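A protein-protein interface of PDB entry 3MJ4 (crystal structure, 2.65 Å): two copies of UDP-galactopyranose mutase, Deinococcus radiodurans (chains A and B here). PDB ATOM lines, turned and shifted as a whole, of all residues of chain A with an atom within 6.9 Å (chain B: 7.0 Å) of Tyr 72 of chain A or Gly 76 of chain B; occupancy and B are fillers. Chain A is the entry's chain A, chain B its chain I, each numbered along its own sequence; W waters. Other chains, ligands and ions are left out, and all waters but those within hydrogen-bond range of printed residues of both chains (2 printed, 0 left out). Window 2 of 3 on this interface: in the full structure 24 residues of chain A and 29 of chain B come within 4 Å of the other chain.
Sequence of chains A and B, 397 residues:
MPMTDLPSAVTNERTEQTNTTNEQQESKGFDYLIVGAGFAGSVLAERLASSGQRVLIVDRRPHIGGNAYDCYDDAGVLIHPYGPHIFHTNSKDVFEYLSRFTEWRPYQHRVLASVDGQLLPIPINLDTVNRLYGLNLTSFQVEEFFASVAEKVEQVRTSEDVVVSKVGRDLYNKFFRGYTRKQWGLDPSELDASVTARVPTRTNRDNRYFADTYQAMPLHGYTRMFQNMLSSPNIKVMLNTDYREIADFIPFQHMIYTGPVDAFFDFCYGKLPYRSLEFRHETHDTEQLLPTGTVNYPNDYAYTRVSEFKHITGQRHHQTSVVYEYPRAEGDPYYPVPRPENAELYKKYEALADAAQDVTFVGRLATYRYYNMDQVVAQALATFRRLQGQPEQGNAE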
ATOM      1  N   TYR A  69     -31.170  32.555 -29.250  1.00  0.00           N
ATOM      2  CA  TYR A  69     -29.920  31.818 -29.190  1.00  0.00           C
ATOM      3  C   TYR A  69     -29.397  31.731 -27.758  1.00  0.00           C
ATOM      4  O   TYR A  69     -29.357  32.739 -27.077  1.00  0.00           O
ATOM      5  CB  TYR A  69     -28.870  32.516 -30.034  1.00  0.00           C
ATOM      6  CG  TYR A  69     -27.535  31.843 -30.001  1.00  0.00           C
ATOM      7  CD1 TYR A  69     -27.371  30.577 -30.544  1.00  0.00           C
ATOM      8  CD2 TYR A  69     -26.439  32.457 -29.438  1.00  0.00           C
ATOM      9  CE1 TYR A  69     -26.152  29.939 -30.520  1.00  0.00           C
ATOM     10  CE2 TYR A  69     -25.213  31.825 -29.405  1.00  0.00           C
ATOM     11  CZ  TYR A  69     -25.083  30.564 -29.947  1.00  0.00           C
ATOM     12  OH  TYR A  69     -23.872  29.920 -29.939  1.00  0.00           O
ATOM     13  N   ASP A  70     -28.984  30.542 -27.318  1.00  0.00           N
ATOM     14  CA  ASP A  70     -28.238  30.410 -26.067  1.00  0.00           C
ATOM     15  C   ASP A  70     -26.955  29.646 -26.242  1.00  0.00           C
ATOM     16  O   ASP A  70     -26.782  28.943 -27.237  1.00  0.00           O
ATOM     17  CB  ASP A  70     -29.074  29.828 -24.898  1.00  0.00           C
ATOM     18  CG  ASP A  70     -29.662  28.426 -25.172  1.00  0.00           C
ATOM     19  OD1 ASP A  70     -30.719  28.134 -24.581  1.00  0.00           O
ATOM     20  OD2 ASP A  70     -29.098  27.602 -25.925  1.00  0.00           O
ATOM     21  N   CYS A  71     -26.057  29.792 -25.274  1.00  0.00           N
ATOM     22  CA  CYS A  71     -24.751  29.148 -25.335  1.00  0.00           C
ATOM     23  C   CYS A  71     -24.061  29.060 -23.965  1.00  0.00           C
ATOM     24  O   CYS A  71     -24.423  29.772 -23.018  1.00  0.00           O
ATOM     25  CB  CYS A  71     -23.858  29.906 -26.311  1.00  0.00           C
ATOM     26  SG  CYS A  71     -23.309  31.498 -25.666  1.00  0.00           S
ATOM     27  N   TYR A  72     -23.067  28.188 -23.849  1.00  0.00           N
ATOM     28  CA  TYR A  72     -22.296  28.124 -22.604  1.00  0.00           C
ATOM     29  C   TYR A  72     -21.203  29.185 -22.615  1.00  0.00           C
ATOM     30  O   TYR A  72     -20.531  29.382 -23.630  1.00  0.00           O
ATOM     31  CB  TYR A  72     -21.697  26.739 -22.375  1.00  0.00           C
ATOM     32  CG  TYR A  72     -22.689  25.718 -21.914  1.00  0.00           C
ATOM     33  CD1 TYR A  72     -22.724  25.302 -20.592  1.00  0.00           C
ATOM     34  CD2 TYR A  72     -23.589  25.161 -22.789  1.00  0.00           C
ATOM     35  CE1 TYR A  72     -23.638  24.357 -20.152  1.00  0.00           C
ATOM     36  CE2 TYR A  72     -24.505  24.229 -22.362  1.00  0.00           C
ATOM     37  CZ  TYR A  72     -24.524  23.826 -21.043  1.00  0.00           C
ATOM     38  OH  TYR A  72     -25.436  22.875 -20.634  1.00  0.00           O
ATOM     39  N   ASP A  73     -21.024  29.871 -21.489  1.00  0.00           N
ATOM     40  CA  ASP A  73     -20.090  30.991 -21.444  1.00  0.00           C
ATOM     41  C   ASP A  73     -18.697  30.543 -21.023  1.00  0.00           C
ATOM     42  O   ASP A  73     -18.430  29.344 -20.910  1.00  0.00           O
ATOM     43  CB  ASP A  73     -20.608  32.107 -20.535  1.00  0.00           C
ATOM     44  CG  ASP A  73     -20.541  31.755 -19.037  1.00  0.00           C
ATOM     45  OD1 ASP A  73     -20.002  30.689 -18.637  1.00  0.00           O
ATOM     46  OD2 ASP A  73     -21.027  32.581 -18.251  1.00  0.00           O
ATOM     47  N   ASP A  74     -17.810  31.507 -20.794  1.00  0.00           N
ATOM     48  CA  ASP A  74     -16.440  31.182 -20.428  1.00  0.00           C
ATOM     49  C   ASP A  74     -16.362  30.353 -19.159  1.00  0.00           C
ATOM     50  O   ASP A  74     -15.392  29.644 -18.950  1.00  0.00           O
ATOM     51  CB  ASP A  74     -15.587  32.441 -20.301  1.00  0.00           C
ATOM     52  CG  ASP A  74     -15.060  32.930 -21.647  1.00  0.00           C
ATOM     53  OD1 ASP A  74     -15.618  32.527 -22.693  1.00  0.00           O
ATOM     54  OD2 ASP A  74     -14.086  33.716 -21.657  1.00  0.00           O
ATOM     55  N   ALA A  75     -17.389  30.416 -18.323  1.00  0.00           N
ATOM     56  CA  ALA A  75     -17.318  29.745 -17.032  1.00  0.00           C
ATOM     57  C   ALA A  75     -18.056  28.404 -17.005  1.00  0.00           C
ATOM     58  O   ALA A  75     -18.052  27.701 -15.984  1.00  0.00           O
ATOM     59  CB  ALA A  75     -17.811  30.665 -15.913  1.00  0.00           C
ATOM     60  N   GLY A  76     -18.677  28.048 -18.124  1.00  0.00           N
ATOM     61  CA  GLY A  76     -19.433  26.814 -18.208  1.00  0.00           C
ATOM     62  C   GLY A  76     -20.877  26.982 -17.774  1.00  0.00           C
ATOM     63  O   GLY A  76     -21.554  26.002 -17.468  1.00  0.00           O
ATOM     64  N   VAL A  77     -21.347  28.226 -17.750  1.00  0.00           N
ATOM     65  CA  VAL A  77     -22.743  28.523 -17.449  1.00  0.00           C
ATOM     66  C   VAL A  77     -23.577  28.787 -18.722  1.00  0.00           C
ATOM     67  O   VAL A  77     -23.288  29.720 -19.475  1.00  0.00           O
ATOM     68  CB  VAL A  77     -22.867  29.767 -16.532  1.00  0.00           C
ATOM     69  CG1 VAL A  77     -24.333  29.982 -16.115  1.00  0.00           C
ATOM     70  CG2 VAL A  77     -21.928  29.659 -15.342  1.00  0.00           C
ATOM     71  N   LEU A  78     -24.604  27.967 -18.946  1.00  0.00           N
ATOM     72  CA  LEU A  78     -25.580  28.202 -19.999  1.00  0.00           C
ATOM     73  C   LEU A  78     -26.202  29.568 -19.815  1.00  0.00           C
ATOM     74  O   LEU A  78     -26.780  29.846 -18.778  1.00  0.00           O
ATOM     75  CB  LEU A  78     -26.684  27.136 -19.965  1.00  0.00           C
ATOM     76  CG  LEU A  78     -27.823  27.263 -20.986  1.00  0.00           C
ATOM     77  CD1 LEU A  78     -27.316  27.156 -22.444  1.00  0.00           C
ATOM     78  CD2 LEU A  78     -28.885  26.229 -20.722  1.00  0.00           C
ATOM     79  N   ILE A  79     -26.091  30.414 -20.834  1.00  0.00           N
ATOM     80  CA  ILE A  79     -26.634  31.774 -20.783  1.00  0.00           C
ATOM     81  C   ILE A  79     -27.377  32.158 -22.059  1.00  0.00           C
ATOM     82  O   ILE A  79     -27.298  31.471 -23.091  1.00  0.00           O
ATOM     83  CB  ILE A  79     -25.526  32.826 -20.610  1.00  0.00           C
ATOM     84  CG1 ILE A  79     -24.646  32.862 -21.861  1.00  0.00           C
ATOM     85  CG2 ILE A  79     -24.698  32.543 -19.395  1.00  0.00           C
ATOM     86  CD1 ILE A  79     -23.528  33.843 -21.749  1.00  0.00           C
ATOM     87  N   HIS A 220     -32.586  21.679 -22.626  1.00  0.00           N
ATOM     88  CA  HIS A 220     -31.158  21.810 -22.894  1.00  0.00           C
ATOM     89  C   HIS A 220     -30.797  23.109 -23.585  1.00  0.00           C
ATOM     90  O   HIS A 220     -29.710  23.237 -24.144  1.00  0.00           O
ATOM     91  CB  HIS A 220     -30.694  20.635 -23.716  1.00  0.00           C
ATOM     92  CG  HIS A 220     -30.992  19.329 -23.072  1.00  0.00           C
ATOM     93  ND1 HIS A 220     -30.281  18.860 -21.989  1.00  0.00           N
ATOM     94  CD2 HIS A 220     -31.947  18.407 -23.325  1.00  0.00           C
ATOM     95  CE1 HIS A 220     -30.767  17.690 -21.623  1.00  0.00           C
ATOM     96  NE2 HIS A 220     -31.777  17.392 -22.419  1.00  0.00           N
ATOM     97  N   ARG A 224     -30.078  23.992 -28.768  1.00  0.00           N
ATOM     98  CA  ARG A 224     -30.333  22.579 -28.980  1.00  0.00           C
ATOM     99  C   ARG A 224     -31.669  22.413 -29.689  1.00  0.00           C
ATOM    100  O   ARG A 224     -31.759  21.666 -30.662  1.00  0.00           O
ATOM    101  CB  ARG A 224     -30.286  21.810 -27.656  1.00  0.00           C
ATOM    102  CG  ARG A 224     -28.874  21.733 -27.094  1.00  0.00           C
ATOM    103  CD  ARG A 224     -28.094  20.581 -27.717  1.00  0.00           C
ATOM    104  NE  ARG A 224     -28.778  19.322 -27.425  1.00  0.00           N
ATOM    105  CZ  ARG A 224     -28.516  18.550 -26.367  1.00  0.00           C
ATOM    106  NH1 ARG A 224     -27.545  18.867 -25.509  1.00  0.00           N
ATOM    107  NH2 ARG A 224     -29.222  17.447 -26.170  1.00  0.00           N
ATOM    108  N   GLN A 315     -29.693  25.064 -14.119  1.00  0.00           N
ATOM    109  CA  GLN A 315     -28.355  24.517 -14.103  1.00  0.00           C
ATOM    110  C   GLN A 315     -27.708  24.639 -12.723  1.00  0.00           C
ATOM    111  O   GLN A 315     -27.766  25.679 -12.088  1.00  0.00           O
ATOM    112  CB  GLN A 315     -27.483  25.179 -15.153  1.00  0.00           C
ATOM    113  CG  GLN A 315     -26.095  24.602 -15.229  1.00  0.00           C
ATOM    114  CD  GLN A 315     -25.102  25.519 -15.941  1.00  0.00           C
ATOM    115  OE1 GLN A 315     -25.444  26.613 -16.387  1.00  0.00           O
ATOM    116  NE2 GLN A 315     -23.862  25.070 -16.037  1.00  0.00           N
ATOM    117  N   HIS A 317     -24.231  24.741 -10.573  1.00  0.00           N
ATOM    118  CA  HIS A 317     -22.925  25.271 -10.901  1.00  0.00           C
ATOM    119  C   HIS A 317     -22.340  25.943  -9.670  1.00  0.00           C
ATOM    120  O   HIS A 317     -23.082  26.515  -8.886  1.00  0.00           O
ATOM    121  CB  HIS A 317     -23.050  26.291 -12.027  1.00  0.00           C
ATOM    122  CG  HIS A 317     -21.778  26.505 -12.786  1.00  0.00           C
ATOM    123  ND1 HIS A 317     -20.737  27.261 -12.294  1.00  0.00           N
ATOM    124  CD2 HIS A 317     -21.374  26.048 -13.997  1.00  0.00           C
ATOM    125  CE1 HIS A 317     -19.748  27.268 -13.176  1.00  0.00           C
ATOM    126  NE2 HIS A 317     -20.113  26.539 -14.216  1.00  0.00           N
ATOM    127  N   CYS B  71     -18.475  20.116 -27.755  1.00  0.00           N
ATOM    128  CA  CYS B  71     -19.732  20.706 -27.318  1.00  0.00           C
ATOM    129  C   CYS B  71     -20.048  20.287 -25.889  1.00  0.00           C
ATOM    130  O   CYS B  71     -19.397  19.397 -25.330  1.00  0.00           O
ATOM    131  CB  CYS B  71     -20.868  20.269 -28.235  1.00  0.00           C
ATOM    132  SG  CYS B  71     -21.228  18.508 -28.130  1.00  0.00           S
ATOM    133  N   TYR B  72     -21.049  20.936 -25.307  1.00  0.00           N
ATOM    134  CA  TYR B  72     -21.530  20.567 -23.976  1.00  0.00           C
ATOM    135  C   TYR B  72     -22.626  19.499 -24.041  1.00  0.00           C
ATOM    136  O   TYR B  72     -23.606  19.658 -24.771  1.00  0.00           O
ATOM    137  CB  TYR B  72     -22.021  21.803 -23.216  1.00  0.00           C
ATOM    138  CG  TYR B  72     -20.898  22.718 -22.793  1.00  0.00           C
ATOM    139  CD1 TYR B  72     -20.309  22.601 -21.527  1.00  0.00           C
ATOM    140  CD2 TYR B  72     -20.407  23.691 -23.661  1.00  0.00           C
ATOM    141  CE1 TYR B  72     -19.260  23.447 -21.135  1.00  0.00           C
ATOM    142  CE2 TYR B  72     -19.363  24.530 -23.287  1.00  0.00           C
ATOM    143  CZ  TYR B  72     -18.790  24.412 -22.028  1.00  0.00           C
ATOM    144  OH  TYR B  72     -17.757  25.264 -21.674  1.00  0.00           O
ATOM    145  N   ASP B  73     -22.460  18.422 -23.271  1.00  0.00           N
ATOM    146  CA  ASP B  73     -23.463  17.361 -23.246  1.00  0.00           C
ATOM    147  C   ASP B  73     -24.685  17.709 -22.396  1.00  0.00           C
ATOM    148  O   ASP B  73     -24.731  18.761 -21.750  1.00  0.00           O
ATOM    149  CB  ASP B  73     -22.854  16.022 -22.799  1.00  0.00           C
ATOM    150  CG  ASP B  73     -22.525  15.960 -21.294  1.00  0.00           C
ATOM    151  OD1 ASP B  73     -22.830  16.903 -20.519  1.00  0.00           O
ATOM    152  OD2 ASP B  73     -21.957  14.926 -20.889  1.00  0.00           O
ATOM    153  N   ASP B  74     -25.668  16.812 -22.409  1.00  0.00           N
ATOM    154  CA  ASP B  74     -26.912  16.967 -21.657  1.00  0.00           C
ATOM    155  C   ASP B  74     -26.728  17.361 -20.182  1.00  0.00           C
ATOM    156  O   ASP B  74     -27.668  17.806 -19.546  1.00  0.00           O
ATOM    157  CB  ASP B  74     -27.750  15.684 -21.749  1.00  0.00           C
ATOM    158  CG  ASP B  74     -28.444  15.519 -23.104  1.00  0.00           C
ATOM    159  OD1 ASP B  74     -28.138  16.298 -24.031  1.00  0.00           O
ATOM    160  OD2 ASP B  74     -29.297  14.605 -23.244  1.00  0.00           O
ATOM    161  N   ALA B  75     -25.517  17.213 -19.655  1.00  0.00           N
ATOM    162  CA  ALA B  75     -25.231  17.457 -18.247  1.00  0.00           C
ATOM    163  C   ALA B  75     -24.385  18.699 -18.030  1.00  0.00           C
ATOM    164  O   ALA B  75     -24.060  19.027 -16.885  1.00  0.00           O
ATOM    165  CB  ALA B  75     -24.507  16.266 -17.656  1.00  0.00           C
ATOM    166  N   GLY B  76     -23.991  19.362 -19.116  1.00  0.00           N
ATOM    167  CA  GLY B  76     -23.179  20.564 -19.025  1.00  0.00           C
ATOM    168  C   GLY B  76     -21.678  20.330 -18.947  1.00  0.00           C
ATOM    169  O   GLY B  76     -20.917  21.253 -18.647  1.00  0.00           O
ATOM    170  N   VAL B  77     -21.261  19.089 -19.203  1.00  0.00           N
ATOM    171  CA  VAL B  77     -19.845  18.719 -19.293  1.00  0.00           C
ATOM    172  C   VAL B  77     -19.316  18.955 -20.710  1.00  0.00           C
ATOM    173  O   VAL B  77     -19.979  18.586 -21.700  1.00  0.00           O
ATOM    174  CB  VAL B  77     -19.654  17.225 -18.994  1.00  0.00           C
ATOM    175  CG1 VAL B  77     -18.172  16.837 -19.109  1.00  0.00           C
ATOM    176  CG2 VAL B  77     -20.243  16.884 -17.624  1.00  0.00           C
ATOM    177  N   LEU B  78     -18.124  19.549 -20.809  1.00  0.00           N
ATOM    178  CA  LEU B  78     -17.518  19.809 -22.116  1.00  0.00           C
ATOM    179  C   LEU B  78     -16.923  18.529 -22.707  1.00  0.00           C
ATOM    180  O   LEU B  78     -15.923  18.026 -22.224  1.00  0.00           O
ATOM    181  CB  LEU B  78     -16.470  20.928 -22.040  1.00  0.00           C
ATOM    182  CG  LEU B  78     -15.707  21.261 -23.332  1.00  0.00           C
ATOM    183  CD1 LEU B  78     -16.646  21.336 -24.511  1.00  0.00           C
ATOM    184  CD2 LEU B  78     -14.925  22.564 -23.215  1.00  0.00           C
ATOM    185  N   ILE B  79     -17.530  18.008 -23.762  1.00  0.00           N
ATOM    186  CA  ILE B  79     -17.043  16.754 -24.323  1.00  0.00           C
ATOM    187  C   ILE B  79     -16.559  16.819 -25.785  1.00  0.00           C
ATOM    188  O   ILE B  79     -16.533  17.880 -26.399  1.00  0.00           O
ATOM    189  CB  ILE B  79     -18.072  15.598 -24.139  1.00  0.00           C
ATOM    190  CG1 ILE B  79     -19.304  15.820 -25.008  1.00  0.00           C
ATOM    191  CG2 ILE B  79     -18.421  15.427 -22.667  1.00  0.00           C
ATOM    192  CD1 ILE B  79     -19.830  14.561 -25.613  1.00  0.00           C
ATOM    193  N   ARG B 224     -14.861  26.851 -30.111  1.00  0.00           N
ATOM    194  CA  ARG B 224     -14.814  28.285 -29.871  1.00  0.00           C
ATOM    195  C   ARG B 224     -13.621  28.831 -30.633  1.00  0.00           C
ATOM    196  O   ARG B 224     -13.655  29.947 -31.157  1.00  0.00           O
ATOM    197  CB  ARG B 224     -14.662  28.588 -28.374  1.00  0.00           C
ATOM    198  CG  ARG B 224     -15.915  28.347 -27.546  1.00  0.00           C
ATOM    199  CD  ARG B 224     -16.745  29.616 -27.410  1.00  0.00           C
ATOM    200  NE  ARG B 224     -15.900  30.707 -26.948  1.00  0.00           N
ATOM    201  CZ  ARG B 224     -15.885  31.179 -25.703  1.00  0.00           C
ATOM    202  NH1 ARG B 224     -16.712  30.679 -24.778  1.00  0.00           N
ATOM    203  NH2 ARG B 224     -15.052  32.170 -25.386  1.00  0.00           N
ATOM    204  N   THR B 283     -22.406   9.572 -18.570  1.00  0.00           N
ATOM    205  CA  THR B 283     -22.238  10.594 -17.526  1.00  0.00           C
ATOM    206  C   THR B 283     -22.435   9.928 -16.188  1.00  0.00           C
ATOM    207  O   THR B 283     -23.378   9.185 -16.013  1.00  0.00           O
ATOM    208  CB  THR B 283     -23.236  11.781 -17.666  1.00  0.00           C
ATOM    209  OG1 THR B 283     -22.958  12.518 -18.864  1.00  0.00           O
ATOM    210  CG2 THR B 283     -23.128  12.716 -16.489  1.00  0.00           C
ATOM    211  N   GLN B 315     -12.219  21.166 -16.823  1.00  0.00           N
ATOM    212  CA  GLN B 315     -13.500  21.665 -16.339  1.00  0.00           C
ATOM    213  C   GLN B 315     -13.794  21.191 -14.916  1.00  0.00           C
ATOM    214  O   GLN B 315     -13.411  20.093 -14.511  1.00  0.00           O
ATOM    215  CB  GLN B 315     -14.645  21.231 -17.274  1.00  0.00           C
ATOM    216  CG  GLN B 315     -16.024  21.703 -16.833  1.00  0.00           C
ATOM    217  CD  GLN B 315     -17.157  21.176 -17.702  1.00  0.00           C
ATOM    218  OE1 GLN B 315     -16.996  20.196 -18.428  1.00  0.00           O
ATOM    219  NE2 GLN B 315     -18.315  21.825 -17.624  1.00  0.00           N
ATOM    220  N   ARG B 316     -14.489  22.027 -14.163  1.00  0.00           N
ATOM    221  CA  ARG B 316     -14.935  21.666 -12.841  1.00  0.00           C
ATOM    222  C   ARG B 316     -16.427  21.415 -12.920  1.00  0.00           C
ATOM    223  O   ARG B 316     -17.150  22.175 -13.570  1.00  0.00           O
ATOM    224  CB  ARG B 316     -14.638  22.807 -11.897  1.00  0.00           C
ATOM    225  CG  ARG B 316     -14.936  22.546 -10.449  1.00  0.00           C
ATOM    226  CD  ARG B 316     -14.441  23.724  -9.647  1.00  0.00           C
ATOM    227  NE  ARG B 316     -14.971  23.729  -8.293  1.00  0.00           N
ATOM    228  CZ  ARG B 316     -14.768  24.724  -7.441  1.00  0.00           C
ATOM    229  NH1 ARG B 316     -14.052  25.776  -7.826  1.00  0.00           N
ATOM    230  NH2 ARG B 316     -15.278  24.672  -6.217  1.00  0.00           N
ATOM    231  N   HIS B 317     -16.889  20.346 -12.260  1.00  0.00           N
ATOM    232  CA  HIS B 317     -18.265  19.861 -12.425  1.00  0.00           C
ATOM    233  C   HIS B 317     -18.616  18.783 -11.386  1.00  0.00           C
ATOM    234  O   HIS B 317     -17.771  17.992 -10.987  1.00  0.00           O
ATOM    235  CB  HIS B 317     -18.443  19.314 -13.853  1.00  0.00           C
ATOM    236  CG  HIS B 317     -19.865  19.214 -14.306  1.00  0.00           C
ATOM    237  ND1 HIS B 317     -20.756  18.303 -13.776  1.00  0.00           N
ATOM    238  CD2 HIS B 317     -20.545  19.895 -15.260  1.00  0.00           C
ATOM    239  CE1 HIS B 317     -21.928  18.443 -14.371  1.00  0.00           C
ATOM    240  NE2 HIS B 317     -21.825  19.397 -15.279  1.00  0.00           N
ATOM    241  N   GLN B 319     -20.735  16.192 -11.715  1.00  0.00           N
ATOM    242  CA  GLN B 319     -20.679  14.886 -12.372  1.00  0.00           C
ATOM    243  C   GLN B 319     -19.473  14.797 -13.310  1.00  0.00           C
ATOM    244  O   GLN B 319     -18.639  15.702 -13.340  1.00  0.00           O
ATOM    245  CB  GLN B 319     -21.961  14.643 -13.144  1.00  0.00           C
ATOM    246  CG  GLN B 319     -23.136  15.384 -12.560  1.00  0.00           C
ATOM    247  CD  GLN B 319     -24.471  14.805 -12.974  1.00  0.00           C
ATOM    248  OE1 GLN B 319     -24.933  14.997 -14.106  1.00  0.00           O
ATOM    249  NE2 GLN B 319     -25.107  14.092 -12.051  1.00  0.00           N
ATOM    250  N   SER B 321     -18.271  13.138 -17.449  1.00  0.00           N
ATOM    251  CA  SER B 321     -18.593  12.442 -18.698  1.00  0.00           C
ATOM    252  C   SER B 321     -17.411  11.722 -19.321  1.00  0.00           C
ATOM    253  O   SER B 321     -16.322  12.296 -19.485  1.00  0.00           O
ATOM    254  CB  SER B 321     -19.198  13.382 -19.730  1.00  0.00           C
ATOM    255  OG  SER B 321     -20.569  13.572 -19.474  1.00  0.00           O
HETATM  256  O   HOH W   1     -25.722  21.372 -25.174  1.00  0.00           O
HETATM  257  O   HOH W   2     -28.482  20.753 -20.839  1.00  0.00           O
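OD1 of Asp 74 of chain B lies within salt-bridge range of NH2 of Arg 224 of chain A (2.7 Å).
The side-chain carboxylate (OD1) of Asp 74 of chain A is in salt-bridge range of the guanidinium group (NH2) of Arg 224 of chain B, 2.8 Å away.
O of Gly 76 of chain B is in hydrogen-bond range of NE2 of Gln 315 of chain B, at 2.9 Å.
OD1 of Asp 73 of chain B sits at hydrogen-bond distance from N of Gly 76 of chain B (3.1 Å).
Among the printed residues, merely in contact across the chains: Tyr 72 of chain A with Tyr 72 of chain B (3.3 Å), His 220 of chain A with Asp 74 of chain B (3.5 Å) and Tyr 72 of chain A with Gly 76 of chain B (3.6 Å).
Tyr 72 of chain A touches just these residues of chain B: Tyr 72 (3.3 Å) and Gly 76 (3.6 Å).
Gly 76 of chain B touches just one residue of chain A: Tyr 72.
Of the printed residues of chain B, His 220 of chain A touches Asp 74 (3.5 Å).
Of the printed residues of chain B, Arg 224 of chain A touches Asp 74.
Of the printed residues of chain A, Asp 74 of chain B touches His 220 (3.5 Å) and Arg 224 (2.7 Å).
The nearest residue of chain B that does not touch Tyr 72 of chain A is Arg 224 of chain B (4.2 Å).
The nearest residue of chain A that does not touch Gly 76 of chain B is Gly 76 of chain A (4.9 Å).
Of the 16 printed residues of chain B, 4 touch a printed residue of chain A.
Printed residues of chain B that touch a printed residue of chain A: Tyr 72, Asp 74, Gly 76 and Arg 224.
Hydrophobic or aromatic side chains of chain A within 4 Å of the printed part of chain B: Tyr 72 and His 220.
Along chain A the printed residues that touch a printed residue of chain B span positions 72 to 224.
Among the printed residues, 5 pairs touch across the chains.
Among the printed residues, Asp or Glu carboxylates within 4 Å of a Lys or Arg side-chain nitrogen of the other chain: Asp 74 of chain A with Arg 224 of chain B (2.8 Å) and Arg 224 of chain A with Asp 74 of chain B (2.7 Å).
Tyr 72 of chain A touches its own counterpart, Tyr 72 of chain B.
Tyr 72 of chain A touches Gly 76 of chain B, but with the chains exchanged Gly 76 of chain A does not touch Tyr 72 of chain B (4.2 Å).
Asp 74 of chain A touches Arg 224 of chain B, and with the chains exchanged Arg 224 of chain A touches Asp 74 of chain B.
Positions printed for both chains: 71, 72, 73, 74, 75, 76, 77, 78, 79, 224, 315 and 317.
Of the 5 pairs that touch across the chains among the printed residues, 3 have their exchanged pair printed and touching as well.
Water W1 bridges the backbone carbonyl oxygen (O) of Tyr 72 of chain B (2.8 Å) and the guanidinium group (NH1) of Arg 224 of chain A (3.1 Å).
Water W2 bridges a ring nitrogen (ND1) of His 220 of chain A (2.9 Å) and the backbone carbonyl oxygen (O) of Asp 74 of chain B (3.3 Å).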
